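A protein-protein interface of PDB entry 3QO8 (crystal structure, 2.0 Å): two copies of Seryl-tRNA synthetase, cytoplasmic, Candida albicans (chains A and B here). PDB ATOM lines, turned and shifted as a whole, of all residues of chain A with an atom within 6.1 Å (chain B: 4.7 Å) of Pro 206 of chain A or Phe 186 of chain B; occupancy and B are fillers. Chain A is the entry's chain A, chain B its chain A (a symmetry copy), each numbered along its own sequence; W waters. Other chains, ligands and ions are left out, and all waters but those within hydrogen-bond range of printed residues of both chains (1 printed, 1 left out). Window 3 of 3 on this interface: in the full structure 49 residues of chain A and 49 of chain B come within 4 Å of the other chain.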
ATOM      1  N   ASN A 193      -0.757   1.315   6.808  1.00  0.00           N
ATOM      2  CA  ASN A 193      -0.135   0.799   8.036  1.00  0.00           C
ATOM      3  C   ASN A 193      -0.311  -0.697   8.260  1.00  0.00           C
ATOM      4  O   ASN A 193       0.606  -1.394   8.726  1.00  0.00           O
ATOM      5  CB  ASN A 193      -0.620   1.595   9.249  1.00  0.00           C
ATOM      6  CG  ASN A 193      -0.092   3.009   9.233  1.00  0.00           C
ATOM      7  OD1 ASN A 193       1.098   3.224   9.042  1.00  0.00           O
ATOM      8  ND2 ASN A 193      -0.970   3.974   9.410  1.00  0.00           N
ATOM      9  N   LEU A 196       2.189  -2.299   5.826  1.00  0.00           N
ATOM     10  CA  LEU A 196       3.561  -2.249   6.343  1.00  0.00           C
ATOM     11  C   LEU A 196       3.758  -3.248   7.476  1.00  0.00           C
ATOM     12  O   LEU A 196       4.767  -3.953   7.534  1.00  0.00           O
ATOM     13  CB  LEU A 196       3.913  -0.836   6.835  1.00  0.00           C
ATOM     14  CG  LEU A 196       4.097   0.204   5.733  1.00  0.00           C
ATOM     15  CD1 LEU A 196       4.255   1.617   6.313  1.00  0.00           C
ATOM     16  CD2 LEU A 196       5.314  -0.161   4.883  1.00  0.00           C
ATOM     17  N   SER A 197       2.786  -3.306   8.381  1.00  0.00           N
ATOM     18  CA  SER A 197       2.883  -4.191   9.538  1.00  0.00           C
ATOM     19  C   SER A 197       2.866  -5.637   9.077  1.00  0.00           C
ATOM     20  O   SER A 197       3.648  -6.475   9.558  1.00  0.00           O
ATOM     21  CB  SER A 197       1.721  -3.941  10.501  1.00  0.00           C
ATOM     22  OG  SER A 197       1.818  -4.777  11.637  1.00  0.00           O
ATOM     23  N   SER A 200       6.167  -6.388   7.357  1.00  0.00           N
ATOM     24  CA  SER A 200       7.232  -6.323   8.352  1.00  0.00           C
ATOM     25  C   SER A 200       7.260  -7.618   9.186  1.00  0.00           C
ATOM     26  O   SER A 200       8.327  -8.126   9.539  1.00  0.00           O
ATOM     27  CB  SER A 200       7.064  -5.076   9.237  1.00  0.00           C
ATOM     28  OG  SER A 200       7.821  -5.191  10.420  1.00  0.00           O
ATOM     29  N   TYR A 204      10.088  -8.312   5.846  1.00  0.00           N
ATOM     30  CA  TYR A 204      10.338  -7.229   4.902  1.00  0.00           C
ATOM     31  C   TYR A 204      10.783  -5.993   5.664  1.00  0.00           C
ATOM     32  O   TYR A 204      10.300  -5.717   6.762  1.00  0.00           O
ATOM     33  CB  TYR A 204       9.074  -6.872   4.116  1.00  0.00           C
ATOM     34  CG  TYR A 204       8.657  -7.865   3.058  1.00  0.00           C
ATOM     35  CD1 TYR A 204       8.590  -7.498   1.717  1.00  0.00           C
ATOM     36  CD2 TYR A 204       8.296  -9.164   3.397  1.00  0.00           C
ATOM     37  CE1 TYR A 204       8.182  -8.415   0.730  1.00  0.00           C
ATOM     38  CE2 TYR A 204       7.900 -10.080   2.425  1.00  0.00           C
ATOM     39  CZ  TYR A 204       7.845  -9.702   1.098  1.00  0.00           C
ATOM     40  OH  TYR A 204       7.443 -10.624   0.140  1.00  0.00           O
ATOM     41  N   VAL A 205      11.698  -5.243   5.071  1.00  0.00           N
ATOM     42  CA  VAL A 205      12.160  -3.989   5.650  1.00  0.00           C
ATOM     43  C   VAL A 205      11.328  -2.824   5.101  1.00  0.00           C
ATOM     44  O   VAL A 205      11.318  -2.587   3.899  1.00  0.00           O
ATOM     45  CB  VAL A 205      13.641  -3.779   5.297  1.00  0.00           C
ATOM     46  CG1 VAL A 205      14.129  -2.402   5.757  1.00  0.00           C
ATOM     47  CG2 VAL A 205      14.482  -4.905   5.900  1.00  0.00           C
ATOM     48  N   PRO A 206      10.627  -2.095   5.984  1.00  0.00           N
ATOM     49  CA  PRO A 206       9.864  -0.935   5.511  1.00  0.00           C
ATOM     50  C   PRO A 206      10.781   0.077   4.864  1.00  0.00           C
ATOM     51  O   PRO A 206      11.841   0.417   5.409  1.00  0.00           O
ATOM     52  CB  PRO A 206       9.253  -0.364   6.793  1.00  0.00           C
ATOM     53  CG  PRO A 206       9.171  -1.557   7.724  1.00  0.00           C
ATOM     54  CD  PRO A 206      10.421  -2.345   7.423  1.00  0.00           C
ATOM     55  N   LEU A 207      10.390   0.559   3.696  1.00  0.00           N
ATOM     56  CA  LEU A 207      11.254   1.497   2.997  1.00  0.00           C
ATOM     57  C   LEU A 207      10.391   2.526   2.301  1.00  0.00           C
ATOM     58  O   LEU A 207       9.701   2.189   1.343  1.00  0.00           O
ATOM     59  CB  LEU A 207      12.106   0.738   1.979  1.00  0.00           C
ATOM     60  CG  LEU A 207      13.218   1.493   1.264  1.00  0.00           C
ATOM     61  CD1 LEU A 207      14.218   2.037   2.280  1.00  0.00           C
ATOM     62  CD2 LEU A 207      13.902   0.587   0.256  1.00  0.00           C
ATOM     63  N   GLN A 208      10.413   3.771   2.778  1.00  0.00           N
ATOM     64  CA  GLN A 208       9.662   4.829   2.109  1.00  0.00           C
ATOM     65  C   GLN A 208      10.527   5.509   1.079  1.00  0.00           C
ATOM     66  O   GLN A 208      11.558   6.101   1.403  1.00  0.00           O
ATOM     67  CB  GLN A 208       9.116   5.866   3.086  1.00  0.00           C
ATOM     68  CG  GLN A 208       8.270   6.957   2.382  1.00  0.00           C
ATOM     69  CD  GLN A 208       7.622   7.906   3.379  1.00  0.00           C
ATOM     70  OE1 GLN A 208       7.309   7.510   4.493  1.00  0.00           O
ATOM     71  NE2 GLN A 208       7.432   9.157   2.987  1.00  0.00           N
ATOM     72  N   ARG A 270      14.364  -8.288   1.235  1.00  0.00           N
ATOM     73  CA  ARG A 270      12.962  -8.014   0.953  1.00  0.00           C
ATOM     74  C   ARG A 270      12.548  -6.644   1.487  1.00  0.00           C
ATOM     75  O   ARG A 270      12.716  -6.369   2.672  1.00  0.00           O
ATOM     76  CB  ARG A 270      12.097  -9.101   1.586  1.00  0.00           C
ATOM     77  CG  ARG A 270      12.470 -10.541   1.136  1.00  0.00           C
ATOM     78  CD  ARG A 270      11.441 -11.547   1.637  1.00  0.00           C
ATOM     79  NE  ARG A 270      11.621 -12.886   1.064  1.00  0.00           N
ATOM     80  CZ  ARG A 270      12.028 -13.946   1.752  1.00  0.00           C
ATOM     81  NH1 ARG A 270      12.291 -13.830   3.048  1.00  0.00           N
ATOM     82  NH2 ARG A 270      12.150 -15.130   1.153  1.00  0.00           N
ATOM     83  N   TYR A 271      12.014  -5.794   0.612  1.00  0.00           N
ATOM     84  CA  TYR A 271      11.555  -4.461   1.014  1.00  0.00           C
ATOM     85  C   TYR A 271      10.030  -4.327   0.915  1.00  0.00           C
ATOM     86  O   TYR A 271       9.422  -4.735  -0.074  1.00  0.00           O
ATOM     87  CB  TYR A 271      12.206  -3.375   0.164  1.00  0.00           C
ATOM     88  CG  TYR A 271      13.693  -3.280   0.385  1.00  0.00           C
ATOM     89  CD1 TYR A 271      14.204  -2.873   1.617  1.00  0.00           C
ATOM     90  CD2 TYR A 271      14.586  -3.621  -0.615  1.00  0.00           C
ATOM     91  CE1 TYR A 271      15.592  -2.800   1.840  1.00  0.00           C
ATOM     92  CE2 TYR A 271      15.958  -3.549  -0.404  1.00  0.00           C
ATOM     93  CZ  TYR A 271      16.451  -3.135   0.822  1.00  0.00           C
ATOM     94  OH  TYR A 271      17.813  -3.072   1.022  1.00  0.00           O
ATOM     95  N   ALA A 272       9.438  -3.771   1.965  1.00  0.00           N
ATOM     96  CA  ALA A 272       8.057  -3.331   1.951  1.00  0.00           C
ATOM     97  C   ALA A 272       8.084  -1.855   1.565  1.00  0.00           C
ATOM     98  O   ALA A 272       8.231  -0.971   2.425  1.00  0.00           O
ATOM     99  CB  ALA A 272       7.438  -3.531   3.320  1.00  0.00           C
ATOM    100  N   GLY A 273       7.970  -1.592   0.266  1.00  0.00           N
ATOM    101  CA  GLY A 273       8.084  -0.240  -0.247  1.00  0.00           C
ATOM    102  C   GLY A 273       6.805   0.534  -0.026  1.00  0.00           C
ATOM    103  O   GLY A 273       5.727  -0.018  -0.143  1.00  0.00           O
ATOM    104  N   LEU B 180      13.226   6.760   3.813  1.00  0.00           N
ATOM    105  CA  LEU B 180      13.080   6.406   5.226  1.00  0.00           C
ATOM    106  C   LEU B 180      13.126   4.890   5.329  1.00  0.00           C
ATOM    107  O   LEU B 180      12.683   4.205   4.408  1.00  0.00           O
ATOM    108  CB  LEU B 180      11.759   6.938   5.790  1.00  0.00           C
ATOM    109  CG  LEU B 180      11.636   8.462   5.795  1.00  0.00           C
ATOM    110  CD1 LEU B 180      10.248   8.847   6.284  1.00  0.00           C
ATOM    111  CD2 LEU B 180      12.721   9.103   6.682  1.00  0.00           C
ATOM    112  N   ARG B 181      13.667   4.360   6.428  1.00  0.00           N
ATOM    113  CA  ARG B 181      13.831   2.906   6.578  1.00  0.00           C
ATOM    114  C   ARG B 181      13.369   2.440   7.948  1.00  0.00           C
ATOM    115  O   ARG B 181      13.569   3.148   8.940  1.00  0.00           O
ATOM    116  CB  ARG B 181      15.317   2.515   6.492  1.00  0.00           C
ATOM    117  CG  ARG B 181      15.958   2.565   5.141  1.00  0.00           C
ATOM    118  CD  ARG B 181      17.463   2.274   5.270  1.00  0.00           C
ATOM    119  NE  ARG B 181      17.715   1.067   6.064  1.00  0.00           N
ATOM    120  CZ  ARG B 181      17.861  -0.159   5.566  1.00  0.00           C
ATOM    121  NH1 ARG B 181      17.788  -0.381   4.252  1.00  0.00           N
ATOM    122  NH2 ARG B 181      18.087  -1.170   6.390  1.00  0.00           N
ATOM    123  N   ASN B 182      12.785   1.244   8.015  1.00  0.00           N
ATOM    124  CA  ASN B 182      12.477   0.644   9.308  1.00  0.00           C
ATOM    125  C   ASN B 182      11.700   1.616  10.187  1.00  0.00           C
ATOM    126  O   ASN B 182      10.642   2.113   9.801  1.00  0.00           O
ATOM    127  CB  ASN B 182      13.775   0.254  10.032  1.00  0.00           C
ATOM    128  CG  ASN B 182      14.531  -0.853   9.329  1.00  0.00           C
ATOM    129  OD1 ASN B 182      13.951  -1.878   8.992  1.00  0.00           O
ATOM    130  ND2 ASN B 182      15.843  -0.656   9.112  1.00  0.00           N
ATOM    131  N   TYR B 183      12.232   1.895  11.373  1.00  0.00           N
ATOM    132  CA  TYR B 183      11.515   2.752  12.311  1.00  0.00           C
ATOM    133  C   TYR B 183      11.412   4.205  11.858  1.00  0.00           C
ATOM    134  O   TYR B 183      10.609   4.969  12.397  1.00  0.00           O
ATOM    135  CB  TYR B 183      12.094   2.644  13.729  1.00  0.00           C
ATOM    136  CG  TYR B 183      11.753   1.333  14.390  1.00  0.00           C
ATOM    137  CD1 TYR B 183      12.717   0.344  14.561  1.00  0.00           C
ATOM    138  CD2 TYR B 183      10.459   1.067  14.816  1.00  0.00           C
ATOM    139  CE1 TYR B 183      12.397  -0.870  15.157  1.00  0.00           C
ATOM    140  CE2 TYR B 183      10.128  -0.142  15.400  1.00  0.00           C
ATOM    141  CZ  TYR B 183      11.101  -1.101  15.572  1.00  0.00           C
ATOM    142  OH  TYR B 183      10.774  -2.296  16.162  1.00  0.00           O
ATOM    143  N   GLY B 184      12.236   4.591  10.889  1.00  0.00           N
ATOM    144  CA  GLY B 184      12.083   5.881  10.251  1.00  0.00           C
ATOM    145  C   GLY B 184      10.713   5.975   9.603  1.00  0.00           C
ATOM    146  O   GLY B 184      10.028   6.986   9.742  1.00  0.00           O
ATOM    147  N   VAL B 185      10.313   4.915   8.899  1.00  0.00           N
ATOM    148  CA  VAL B 185       8.993   4.864   8.271  1.00  0.00           C
ATOM    149  C   VAL B 185       7.918   4.828   9.347  1.00  0.00           C
ATOM    150  O   VAL B 185       6.948   5.570   9.269  1.00  0.00           O
ATOM    151  CB  VAL B 185       8.821   3.626   7.358  1.00  0.00           C
ATOM    152  CG1 VAL B 185       7.403   3.622   6.715  1.00  0.00           C
ATOM    153  CG2 VAL B 185       9.919   3.575   6.267  1.00  0.00           C
ATOM    154  N   PHE B 186       8.094   3.970  10.355  1.00  0.00           N
ATOM    155  CA  PHE B 186       7.073   3.801  11.397  1.00  0.00           C
ATOM    156  C   PHE B 186       6.844   5.086  12.210  1.00  0.00           C
ATOM    157  O   PHE B 186       5.712   5.420  12.569  1.00  0.00           O
ATOM    158  CB  PHE B 186       7.430   2.649  12.336  1.00  0.00           C
ATOM    159  CG  PHE B 186       7.252   1.275  11.725  1.00  0.00           C
ATOM    160  CD1 PHE B 186       6.213   1.014  10.852  1.00  0.00           C
ATOM    161  CD2 PHE B 186       8.129   0.245  12.042  1.00  0.00           C
ATOM    162  CE1 PHE B 186       6.036  -0.256  10.304  1.00  0.00           C
ATOM    163  CE2 PHE B 186       7.962  -1.036  11.493  1.00  0.00           C
ATOM    164  CZ  PHE B 186       6.923  -1.279  10.624  1.00  0.00           C
ATOM    165  N   LEU B 187       7.917   5.816  12.492  1.00  0.00           N
ATOM    166  CA  LEU B 187       7.777   7.067  13.233  1.00  0.00           C
ATOM    167  C   LEU B 187       7.054   8.122  12.403  1.00  0.00           C
ATOM    168  O   LEU B 187       6.257   8.889  12.927  1.00  0.00           O
ATOM    169  CB  LEU B 187       9.144   7.613  13.661  1.00  0.00           C
ATOM    170  CG  LEU B 187       9.736   6.963  14.915  1.00  0.00           C
ATOM    171  CD1 LEU B 187      11.228   7.233  15.017  1.00  0.00           C
ATOM    172  CD2 LEU B 187       8.991   7.434  16.159  1.00  0.00           C
ATOM    173  N   ASN B 188       7.381   8.195  11.118  1.00  0.00           N
ATOM    174  CA  ASN B 188       6.708   9.139  10.240  1.00  0.00           C
ATOM    175  C   ASN B 188       5.203   8.860  10.180  1.00  0.00           C
ATOM    176  O   ASN B 188       4.391   9.763  10.355  1.00  0.00           O
ATOM    177  CB  ASN B 188       7.330   9.118   8.848  1.00  0.00           C
ATOM    178  CG  ASN B 188       7.074  10.401   8.087  1.00  0.00           C
ATOM    179  OD1 ASN B 188       7.466  11.491   8.523  1.00  0.00           O
ATOM    180  ND2 ASN B 188       6.456  10.279   6.931  1.00  0.00           N
ATOM    181  N   GLN B 189       4.840   7.593   9.969  1.00  0.00           N
ATOM    182  CA  GLN B 189       3.433   7.194   9.970  1.00  0.00           C
ATOM    183  C   GLN B 189       2.769   7.445  11.323  1.00  0.00           C
ATOM    184  O   GLN B 189       1.611   7.869  11.386  1.00  0.00           O
ATOM    185  CB  GLN B 189       3.293   5.723   9.557  1.00  0.00           C
ATOM    186  CG  GLN B 189       3.538   5.492   8.060  1.00  0.00           C
ATOM    187  CD  GLN B 189       2.541   6.238   7.197  1.00  0.00           C
ATOM    188  OE1 GLN B 189       2.911   7.014   6.317  1.00  0.00           O
ATOM    189  NE2 GLN B 189       1.267   6.000   7.442  1.00  0.00           N
ATOM    190  N   ALA B 190       3.501   7.176  12.405  1.00  0.00           N
ATOM    191  CA  ALA B 190       2.989   7.420  13.742  1.00  0.00           C
ATOM    192  C   ALA B 190       2.584   8.883  13.884  1.00  0.00           C
ATOM    193  O   ALA B 190       1.500   9.184  14.368  1.00  0.00           O
ATOM    194  CB  ALA B 190       4.046   7.029  14.829  1.00  0.00           C
ATOM    195  N   ILE B 435       2.799   2.226  16.388  1.00  0.00           N
ATOM    196  CA  ILE B 435       3.951   1.513  15.860  1.00  0.00           C
ATOM    197  C   ILE B 435       3.809   0.023  16.168  1.00  0.00           C
ATOM    198  O   ILE B 435       3.517  -0.355  17.304  1.00  0.00           O
ATOM    199  CB  ILE B 435       5.250   2.058  16.481  1.00  0.00           C
ATOM    200  CG1 ILE B 435       5.433   3.539  16.097  1.00  0.00           C
ATOM    201  CG2 ILE B 435       6.460   1.205  16.071  1.00  0.00           C
ATOM    202  CD1 ILE B 435       6.598   4.226  16.867  1.00  0.00           C
ATOM    203  N   PRO B 436       4.004  -0.828  15.154  1.00  0.00           N
ATOM    204  CA  PRO B 436       3.894  -2.279  15.370  1.00  0.00           C
ATOM    205  C   PRO B 436       4.809  -2.736  16.506  1.00  0.00           C
ATOM    206  O   PRO B 436       5.989  -2.400  16.527  1.00  0.00           O
ATOM    207  CB  PRO B 436       4.369  -2.867  14.038  1.00  0.00           C
ATOM    208  CG  PRO B 436       4.080  -1.787  13.027  1.00  0.00           C
ATOM    209  CD  PRO B 436       4.354  -0.494  13.763  1.00  0.00           C
HETATM  210  O   HOH W   1       5.525   7.616   6.260  1.00  0.00           O
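NE2 of Gln 189 of chain B is in hydrogen-bond range of OD1 of Asn 193 of chain A. The backbone carbonyl oxygen of Pro 206 of chain A sits at hydrogen-bond distance from the backbone NH of Asn 182 of chain B (2.9 Å). N of Gln 208 of chain A lies within hydrogen-bond range of O of Leu 180 of chain B, at 2.8 Å.
N of Val 205 of chain A is in hydrogen-bond range of O of Arg 270 of chain A (2.8 Å). O of Val 205 of chain A lies within hydrogen-bond range of N of Ala 272 of chain A, at 2.9 Å. The backbone NH (N) of Leu 207 of chain A is in hydrogen-bond range of the backbone carbonyl oxygen (O) of Ala 272 of chain A, 2.9 Å away.
Among the printed residues, pairs that only touch across the chains: Leu 196 of chain A with Val 185 of chain B (3.8 Å), Ser 197 of chain A with Pro 436 of chain B (3.99 Å), Val 205 of chain A with Asn 182 of chain B (3.3 Å), Pro 206 of chain A with Arg 181 of chain B (3.4 Å), Pro 206 of chain A with Val 185 of chain B (3.8 Å), Pro 206 of chain A with Phe 186 of chain B (3.7 Å), Leu 207 of chain A with Leu 180 of chain B (3.4 Å), Leu 207 of chain A with Arg 181 of chain B (3.4 Å), Leu 207 of chain A with Val 185 of chain B (3.99 Å), Gln 208 of chain A with Val 185 of chain B (3.5 Å) and Gln 208 of chain A with Asn 188 of chain B (3.8 Å).
Of the printed residues of chain A, Phe 186 of chain B touches Pro 206 (3.7 Å). Printed residues of chain B within 4 Å of Gln 208 of chain A: Leu 180, Val 185 and Asn 188. Of the printed residues of chain A, Arg 181 of chain B touches Pro 206 and Leu 207. Printed residues of chain A within 4 Å of Val 185 of chain B: Leu 196 (3.8 Å), Pro 206 (3.8 Å), Leu 207 (3.99 Å) and Gln 208 (3.5 Å). Of the printed residues of chain B, Ser 197 of chain A touches Pro 436. Of the printed residues of chain A, Asn 182 of chain B touches Val 205 and Pro 206. The nearest printed residue of chain B that does not touch Pro 206 of chain A is Leu 180 of chain B (4.01 Å). The nearest printed residue of chain A that does not touch Phe 186 of chain B is Ser 200 of chain A (4.02 Å).
Hydrophobic or aromatic side chains of chain B within 4 Å of the printed part of chain A: Leu 180, Val 185, Phe 186 and Pro 436. Hydrophobic or aromatic side chains of chain A within 4 Å of the printed part of chain B: Leu 196, Val 205, Pro 206 and Leu 207.
No position is printed for both chains. Of the 14 pairs that touch across the chains among the printed residues, none has its exchanged pair printed and touching as well.
Water W1 lies within hydrogen-bond range of OE1 of Gln 208 of chain A (2.5 Å), OE1 of Gln 189 of chain B (2.7 Å) and ND2 of Asn 188 of chain B (2.9 Å).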
